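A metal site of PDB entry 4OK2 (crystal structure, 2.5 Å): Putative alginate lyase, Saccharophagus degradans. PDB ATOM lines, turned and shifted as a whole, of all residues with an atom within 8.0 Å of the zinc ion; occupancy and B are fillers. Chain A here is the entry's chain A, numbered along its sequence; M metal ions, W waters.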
ATOM      1  N   PRO A 308      25.733  -3.000  -3.525  1.00  0.00           N
ATOM      2  CA  PRO A 308      24.390  -3.501  -3.759  1.00  0.00           C
ATOM      3  C   PRO A 308      23.353  -2.800  -2.886  1.00  0.00           C
ATOM      4  O   PRO A 308      22.640  -3.479  -2.123  1.00  0.00           O
ATOM      5  CB  PRO A 308      24.506  -4.962  -3.350  1.00  0.00           C
ATOM      6  CG  PRO A 308      25.561  -4.982  -2.303  1.00  0.00           C
ATOM      7  CD  PRO A 308      26.539  -3.917  -2.700  1.00  0.00           C
ATOM      8  N   ILE A 309      23.261  -1.485  -3.004  1.00  0.00           N
ATOM      9  CA  ILE A 309      22.280  -0.681  -2.237  1.00  0.00           C
ATOM     10  C   ILE A 309      21.001  -0.534  -3.057  1.00  0.00           C
ATOM     11  O   ILE A 309      21.066  -0.510  -4.291  1.00  0.00           O
ATOM     12  CB  ILE A 309      22.832   0.710  -1.893  1.00  0.00           C
ATOM     13  CG1 ILE A 309      23.098   1.520  -3.156  1.00  0.00           C
ATOM     14  CG2 ILE A 309      24.136   0.594  -1.146  1.00  0.00           C
ATOM     15  CD1 ILE A 309      23.424   2.971  -2.876  1.00  0.00           C
ATOM     16  N   ASN A 310      19.851  -0.429  -2.386  1.00  0.00           N
ATOM     17  CA  ASN A 310      18.561  -0.457  -3.086  1.00  0.00           C
ATOM     18  C   ASN A 310      18.359  -1.754  -3.881  1.00  0.00           C
ATOM     19  O   ASN A 310      18.902  -2.785  -3.498  1.00  0.00           O
ATOM     20  CB  ASN A 310      18.387   0.808  -3.941  1.00  0.00           C
ATOM     21  CG  ASN A 310      18.339   2.069  -3.079  1.00  0.00           C
ATOM     22  OD1 ASN A 310      17.892   2.017  -1.958  1.00  0.00           O
ATOM     23  ND2 ASN A 310      18.770   3.200  -3.615  1.00  0.00           N
ATOM     24  N   ASP A 311      17.558  -1.742  -4.941  1.00  0.00           N
ATOM     25  CA  ASP A 311      17.300  -2.982  -5.702  1.00  0.00           C
ATOM     26  C   ASP A 311      18.454  -3.321  -6.622  1.00  0.00           C
ATOM     27  O   ASP A 311      18.611  -2.725  -7.674  1.00  0.00           O
ATOM     28  CB  ASP A 311      15.994  -2.885  -6.508  1.00  0.00           C
ATOM     29  CG  ASP A 311      14.760  -3.274  -5.683  1.00  0.00           C
ATOM     30  OD1 ASP A 311      14.904  -3.677  -4.492  1.00  0.00           O
ATOM     31  OD2 ASP A 311      13.631  -3.177  -6.232  1.00  0.00           O
ATOM     32  N   ALA A 312      19.250  -4.298  -6.247  1.00  0.00           N
ATOM     33  CA  ALA A 312      20.531  -4.588  -6.905  1.00  0.00           C
ATOM     34  C   ALA A 312      20.813  -6.091  -6.816  1.00  0.00           C
ATOM     35  O   ALA A 312      20.490  -6.705  -5.814  1.00  0.00           O
ATOM     36  CB  ALA A 312      21.639  -3.809  -6.218  1.00  0.00           C
ATOM     37  N   LYS A 405      25.085   5.411   3.398  1.00  0.00           N
ATOM     38  CA  LYS A 405      23.959   5.632   2.503  1.00  0.00           C
ATOM     39  C   LYS A 405      22.970   6.606   3.140  1.00  0.00           C
ATOM     40  O   LYS A 405      21.968   6.224   3.766  1.00  0.00           O
ATOM     41  CB  LYS A 405      23.293   4.295   2.149  1.00  0.00           C
ATOM     42  CG  LYS A 405      22.253   4.455   1.073  1.00  0.00           C
ATOM     43  CD  LYS A 405      21.484   3.180   0.812  1.00  0.00           C
ATOM     44  CE  LYS A 405      20.022   3.516   0.594  1.00  0.00           C
ATOM     45  NZ  LYS A 405      19.594   3.070  -0.747  1.00  0.00           N
ATOM     46  N   HIS A 413      12.245   1.296  -6.402  1.00  0.00           N
ATOM     47  CA  HIS A 413      13.357   0.388  -6.197  1.00  0.00           C
ATOM     48  C   HIS A 413      14.156   0.641  -4.907  1.00  0.00           C
ATOM     49  O   HIS A 413      15.007  -0.179  -4.519  1.00  0.00           O
ATOM     50  CB  HIS A 413      14.250   0.394  -7.433  1.00  0.00           C
ATOM     51  CG  HIS A 413      13.646  -0.332  -8.606  1.00  0.00           C
ATOM     52  ND1 HIS A 413      13.540  -1.710  -8.645  1.00  0.00           N
ATOM     53  CD2 HIS A 413      13.120   0.117  -9.767  1.00  0.00           C
ATOM     54  CE1 HIS A 413      12.965  -2.070  -9.775  1.00  0.00           C
ATOM     55  NE2 HIS A 413      12.695  -0.984 -10.471  1.00  0.00           N
ATOM     56  N   GLY A 414      13.877   1.750  -4.229  1.00  0.00           N
ATOM     57  CA  GLY A 414      14.640   2.167  -3.072  1.00  0.00           C
ATOM     58  C   GLY A 414      14.313   1.373  -1.829  1.00  0.00           C
ATOM     59  O   GLY A 414      13.203   0.887  -1.662  1.00  0.00           O
ATOM     60  N   HIS A 415      15.301   1.212  -0.952  1.00  0.00           N
ATOM     61  CA  HIS A 415      15.120   0.487   0.285  1.00  0.00           C
ATOM     62  C   HIS A 415      14.854   1.384   1.496  1.00  0.00           C
ATOM     63  O   HIS A 415      15.259   2.570   1.513  1.00  0.00           O
ATOM     64  CB  HIS A 415      16.316  -0.411   0.501  1.00  0.00           C
ATOM     65  CG  HIS A 415      16.343  -1.582  -0.420  1.00  0.00           C
ATOM     66  ND1 HIS A 415      17.273  -2.592  -0.317  1.00  0.00           N
ATOM     67  CD2 HIS A 415      15.541  -1.900  -1.473  1.00  0.00           C
ATOM     68  CE1 HIS A 415      17.039  -3.486  -1.267  1.00  0.00           C
ATOM     69  NE2 HIS A 415      15.998  -3.089  -1.972  1.00  0.00           N
ATOM     70  N   PHE A 416      14.171   0.834   2.496  1.00  0.00           N
ATOM     71  CA  PHE A 416      13.832   1.579   3.707  1.00  0.00           C
ATOM     72  C   PHE A 416      14.958   1.578   4.735  1.00  0.00           C
ATOM     73  O   PHE A 416      14.836   1.000   5.821  1.00  0.00           O
ATOM     74  CB  PHE A 416      12.512   1.069   4.261  1.00  0.00           C
ATOM     75  CG  PHE A 416      11.372   1.239   3.296  1.00  0.00           C
ATOM     76  CD1 PHE A 416      10.780   2.474   3.110  1.00  0.00           C
ATOM     77  CD2 PHE A 416      10.918   0.164   2.547  1.00  0.00           C
ATOM     78  CE1 PHE A 416       9.746   2.636   2.193  1.00  0.00           C
ATOM     79  CE2 PHE A 416       9.886   0.317   1.629  1.00  0.00           C
ATOM     80  CZ  PHE A 416       9.298   1.563   1.452  1.00  0.00           C
ATOM     81  N   ASP A 417      16.056   2.247   4.389  1.00  0.00           N
ATOM     82  CA  ASP A 417      17.302   2.056   5.102  1.00  0.00           C
ATOM     83  C   ASP A 417      18.114   3.337   5.253  1.00  0.00           C
ATOM     84  O   ASP A 417      19.315   3.364   5.028  1.00  0.00           O
ATOM     85  CB  ASP A 417      18.128   0.940   4.417  1.00  0.00           C
ATOM     86  CG  ASP A 417      18.551   1.285   2.961  1.00  0.00           C
ATOM     87  OD1 ASP A 417      17.929   2.155   2.319  1.00  0.00           O
ATOM     88  OD2 ASP A 417      19.503   0.666   2.443  1.00  0.00           O
ATOM     89  N   ASN A 420      21.993   3.839   6.414  1.00  0.00           N
ATOM     90  CA  ASN A 420      22.533   2.489   6.390  1.00  0.00           C
ATOM     91  C   ASN A 420      24.037   2.568   6.056  1.00  0.00           C
ATOM     92  O   ASN A 420      24.504   3.592   5.557  1.00  0.00           O
ATOM     93  CB  ASN A 420      21.778   1.676   5.342  1.00  0.00           C
ATOM     94  CG  ASN A 420      22.329   0.276   5.165  1.00  0.00           C
ATOM     95  OD1 ASN A 420      22.700  -0.388   6.131  1.00  0.00           O
ATOM     96  ND2 ASN A 420      22.352  -0.185   3.926  1.00  0.00           N
ATOM     97  N   LEU A 422      27.652   0.034   4.725  1.00  0.00           N
ATOM     98  CA  LEU A 422      28.321  -1.176   4.272  1.00  0.00           C
ATOM     99  C   LEU A 422      29.796  -0.949   4.469  1.00  0.00           C
ATOM    100  O   LEU A 422      30.282   0.186   4.468  1.00  0.00           O
ATOM    101  CB  LEU A 422      28.151  -1.350   2.763  1.00  0.00           C
ATOM    102  CG  LEU A 422      26.777  -1.590   2.141  1.00  0.00           C
ATOM    103  CD1 LEU A 422      25.908  -0.342   2.124  1.00  0.00           C
ATOM    104  CD2 LEU A 422      26.990  -2.054   0.711  1.00  0.00           C
ATOM    105  N   THR A 432      27.237  -5.918   5.287  1.00  0.00           N
ATOM    106  CA  THR A 432      26.646  -6.149   3.988  1.00  0.00           C
ATOM    107  C   THR A 432      25.279  -5.551   3.740  1.00  0.00           C
ATOM    108  O   THR A 432      24.566  -5.195   4.679  1.00  0.00           O
ATOM    109  CB  THR A 432      26.577  -7.659   3.712  1.00  0.00           C
ATOM    110  OG1 THR A 432      25.682  -8.269   4.653  1.00  0.00           O
ATOM    111  CG2 THR A 432      27.973  -8.255   3.864  1.00  0.00           C
ATOM    112  N   ASP A 433      24.924  -5.465   2.461  1.00  0.00           N
ATOM    113  CA  ASP A 433      23.574  -5.079   2.039  1.00  0.00           C
ATOM    114  C   ASP A 433      23.053  -6.259   1.216  1.00  0.00           C
ATOM    115  O   ASP A 433      23.797  -6.852   0.410  1.00  0.00           O
ATOM    116  CB  ASP A 433      23.606  -3.786   1.240  1.00  0.00           C
ATOM    117  CG  ASP A 433      22.265  -3.060   1.207  1.00  0.00           C
ATOM    118  OD1 ASP A 433      21.205  -3.686   1.154  1.00  0.00           O
ATOM    119  OD2 ASP A 433      22.283  -1.804   1.190  1.00  0.00           O
ATOM    120  N   TYR A 434      21.809  -6.629   1.456  1.00  0.00           N
ATOM    121  CA  TYR A 434      21.257  -7.819   0.872  1.00  0.00           C
ATOM    122  C   TYR A 434      21.044  -7.694  -0.644  1.00  0.00           C
ATOM    123  O   TYR A 434      21.062  -8.683  -1.343  1.00  0.00           O
ATOM    124  CB  TYR A 434      19.944  -8.190   1.554  1.00  0.00           C
ATOM    125  CG  TYR A 434      19.473  -9.581   1.212  1.00  0.00           C
ATOM    126  CD1 TYR A 434      18.612  -9.799   0.138  1.00  0.00           C
ATOM    127  CD2 TYR A 434      19.915 -10.679   1.956  1.00  0.00           C
ATOM    128  CE1 TYR A 434      18.205 -11.092  -0.202  1.00  0.00           C
ATOM    129  CE2 TYR A 434      19.517 -11.959   1.632  1.00  0.00           C
ATOM    130  CZ  TYR A 434      18.660 -12.156   0.554  1.00  0.00           C
ATOM    131  OH  TYR A 434      18.278 -13.443   0.232  1.00  0.00           O
ATOM    132  N   GLY A 435      20.812  -6.485  -1.146  1.00  0.00           N
ATOM    133  CA  GLY A 435      20.426  -6.349  -2.546  1.00  0.00           C
ATOM    134  C   GLY A 435      18.973  -6.725  -2.739  1.00  0.00           C
ATOM    135  O   GLY A 435      18.163  -6.621  -1.819  1.00  0.00           O
ATOM    136  N   ALA A 436      18.621  -7.180  -3.936  1.00  0.00           N
ATOM    137  CA  ALA A 436      17.273  -7.566  -4.232  1.00  0.00           C
ATOM    138  C   ALA A 436      17.062  -9.066  -4.037  1.00  0.00           C
ATOM    139  O   ALA A 436      18.007  -9.837  -4.091  1.00  0.00           O
ATOM    140  CB  ALA A 436      16.910  -7.154  -5.648  1.00  0.00           C
ATOM    141  N   ASN A 454      11.200  -9.747  -1.941  1.00  0.00           N
ATOM    142  CA  ASN A 454      11.771  -8.421  -2.193  1.00  0.00           C
ATOM    143  C   ASN A 454      11.161  -7.257  -1.401  1.00  0.00           C
ATOM    144  O   ASN A 454      11.889  -6.398  -0.917  1.00  0.00           O
ATOM    145  CB  ASN A 454      11.804  -8.060  -3.674  1.00  0.00           C
ATOM    146  CG  ASN A 454      12.863  -7.022  -3.964  1.00  0.00           C
ATOM    147  OD1 ASN A 454      14.026  -7.194  -3.581  1.00  0.00           O
ATOM    148  ND2 ASN A 454      12.483  -5.935  -4.615  1.00  0.00           N
ATOM    149  N   TRP A 457      11.102  -8.758   2.601  1.00  0.00           N
ATOM    150  CA  TRP A 457      12.372  -8.692   3.274  1.00  0.00           C
ATOM    151  C   TRP A 457      13.389  -7.664   2.778  1.00  0.00           C
ATOM    152  O   TRP A 457      13.819  -6.803   3.548  1.00  0.00           O
ATOM    153  CB  TRP A 457      13.046 -10.056   3.365  1.00  0.00           C
ATOM    154  CG  TRP A 457      13.961 -10.018   4.572  1.00  0.00           C
ATOM    155  CD1 TRP A 457      13.591  -9.907   5.902  1.00  0.00           C
ATOM    156  CD2 TRP A 457      15.358 -10.015   4.554  1.00  0.00           C
ATOM    157  NE1 TRP A 457      14.705  -9.858   6.719  1.00  0.00           N
ATOM    158  CE2 TRP A 457      15.806  -9.927   5.916  1.00  0.00           C
ATOM    159  CE3 TRP A 457      16.284 -10.115   3.534  1.00  0.00           C
ATOM    160  CZ2 TRP A 457      17.130  -9.921   6.255  1.00  0.00           C
ATOM    161  CZ3 TRP A 457      17.583 -10.096   3.878  1.00  0.00           C
ATOM    162  CH2 TRP A 457      18.008 -10.003   5.231  1.00  0.00           C
ATOM    163  N   ALA A 458      13.792  -7.769   1.509  1.00  0.00           N
ATOM    164  CA  ALA A 458      14.952  -7.015   1.042  1.00  0.00           C
ATOM    165  C   ALA A 458      14.849  -5.507   1.296  1.00  0.00           C
ATOM    166  O   ALA A 458      15.843  -4.872   1.636  1.00  0.00           O
ATOM    167  CB  ALA A 458      15.207  -7.302  -0.418  1.00  0.00           C
ATOM    168  N   LYS A 459      13.659  -4.941   1.146  1.00  0.00           N
ATOM    169  CA  LYS A 459      13.441  -3.499   1.331  1.00  0.00           C
ATOM    170  C   LYS A 459      13.371  -3.061   2.783  1.00  0.00           C
ATOM    171  O   LYS A 459      13.572  -1.891   3.080  1.00  0.00           O
ATOM    172  CB  LYS A 459      12.160  -3.049   0.623  1.00  0.00           C
ATOM    173  CG  LYS A 459      12.218  -3.197  -0.884  1.00  0.00           C
ATOM    174  CD  LYS A 459      10.957  -2.692  -1.564  1.00  0.00           C
ATOM    175  CE  LYS A 459      11.194  -2.619  -3.059  1.00  0.00           C
ATOM    176  NZ  LYS A 459      10.082  -1.990  -3.817  1.00  0.00           N
ATOM    177  N   GLN A 460      13.075  -3.993   3.681  1.00  0.00           N
ATOM    178  CA  GLN A 460      12.741  -3.628   5.053  1.00  0.00           C
ATOM    179  C   GLN A 460      13.968  -3.219   5.850  1.00  0.00           C
ATOM    180  O   GLN A 460      15.056  -3.781   5.675  1.00  0.00           O
ATOM    181  CB  GLN A 460      11.965  -4.762   5.747  1.00  0.00           C
ATOM    182  CG  GLN A 460      10.702  -5.216   5.020  1.00  0.00           C
ATOM    183  CD  GLN A 460       9.658  -4.104   4.812  1.00  0.00           C
ATOM    184  OE1 GLN A 460       9.049  -4.002   3.747  1.00  0.00           O
ATOM    185  NE2 GLN A 460       9.460  -3.251   5.828  1.00  0.00           N
ATOM    186  N   ALA A 463      16.369  -5.643   7.565  1.00  0.00           N
ATOM    187  CA  ALA A 463      17.309  -6.337   6.688  1.00  0.00           C
ATOM    188  C   ALA A 463      18.574  -5.519   6.461  1.00  0.00           C
ATOM    189  O   ALA A 463      19.464  -5.945   5.737  1.00  0.00           O
ATOM    190  CB  ALA A 463      16.650  -6.624   5.347  1.00  0.00           C
ATOM    191  N   HIS A 464      18.652  -4.337   7.088  1.00  0.00           N
ATOM    192  CA  HIS A 464      19.732  -3.378   6.829  1.00  0.00           C
ATOM    193  C   HIS A 464      20.461  -3.019   8.121  1.00  0.00           C
ATOM    194  O   HIS A 464      19.928  -3.215   9.212  1.00  0.00           O
ATOM    195  CB  HIS A 464      19.161  -2.112   6.185  1.00  0.00           C
ATOM    196  CG  HIS A 464      18.750  -2.310   4.760  1.00  0.00           C
ATOM    197  ND1 HIS A 464      17.482  -2.744   4.398  1.00  0.00           N
ATOM    198  CD2 HIS A 464      19.434  -2.154   3.598  1.00  0.00           C
ATOM    199  CE1 HIS A 464      17.410  -2.832   3.081  1.00  0.00           C
ATOM    200  NE2 HIS A 464      18.576  -2.468   2.573  1.00  0.00           N
ATOM    201  N   ASN A 465      21.681  -2.496   7.991  1.00  0.00           N
ATOM    202  CA  ASN A 465      22.492  -2.119   9.143  1.00  0.00           C
ATOM    203  C   ASN A 465      22.164  -0.747   9.710  1.00  0.00           C
ATOM    204  O   ASN A 465      23.052   0.091   9.825  1.00  0.00           O
ATOM    205  CB  ASN A 465      23.952  -2.120   8.740  1.00  0.00           C
ATOM    206  CG  ASN A 465      24.338  -3.411   8.095  1.00  0.00           C
ATOM    207  OD1 ASN A 465      24.153  -4.473   8.688  1.00  0.00           O
ATOM    208  ND2 ASN A 465      24.841  -3.338   6.853  1.00  0.00           N
HETATM  209 ZN    ZN M   1      19.186  -3.019   0.619  1.00  0.00          ZN
HETATM  210  O   HOH W   1      19.855  -1.257   0.574  1.00  0.00           O
HETATM  211  O   HOH W   2      20.002  -3.404  -1.526  1.00  0.00           O
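NE2 of His 464 sits close to OD2 of Asp 417 (3.3 Å). A ring nitrogen (ND1) of His 464 sits at hydrogen-bond distance from the backbone carbonyl oxygen (O) of Gln 460. A ring nitrogen (ND1) of His 415 sits close to the backbone carbonyl oxygen of Ala 458 (3.3 Å). OD1 of Asn 310 sits at hydrogen-bond distance from N of His 415 (2.9 Å). A ring nitrogen (NE2) of His 415 is in hydrogen-bond range of the side-chain carboxylate (OD1) of Asp 311 (2.8 Å). OD2 of Asp 433 sits at hydrogen-bond distance from ND2 of Asn 420 (3.2 Å).
Residues that only touch the zinc ion: Ala 458 (3.96 Å). Of the 26 residues printed, 4 come within 4 Å of the zinc ion. Along chain A the residues within 4 Å of the zinc ion span positions 415 to 464.
The zinc ion is bound by water W1 (1.9 Å), a ring nitrogen (NE2) of His 464 (2.1 Å), a ring nitrogen (ND1) of His 415 (2.2 Å), the side-chain carboxylate (OD1) of Asp 433 (2.2 Å) and water W2 (2.3 Å).
Water W1 lies within hydrogen-bond range of the side-chain carboxylate (OD2) of Asp 433 (2.6 Å), the side-chain carboxylate (OD2) of Asp 417 (2.7 Å) and the backbone NH (N) of Asn 310 (3.1 Å). Water W2 lies within hydrogen-bond range of O of Pro 308 (2.7 Å), N of Asn 310 (3.1 Å) and N of Gly 435 (3.2 Å).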
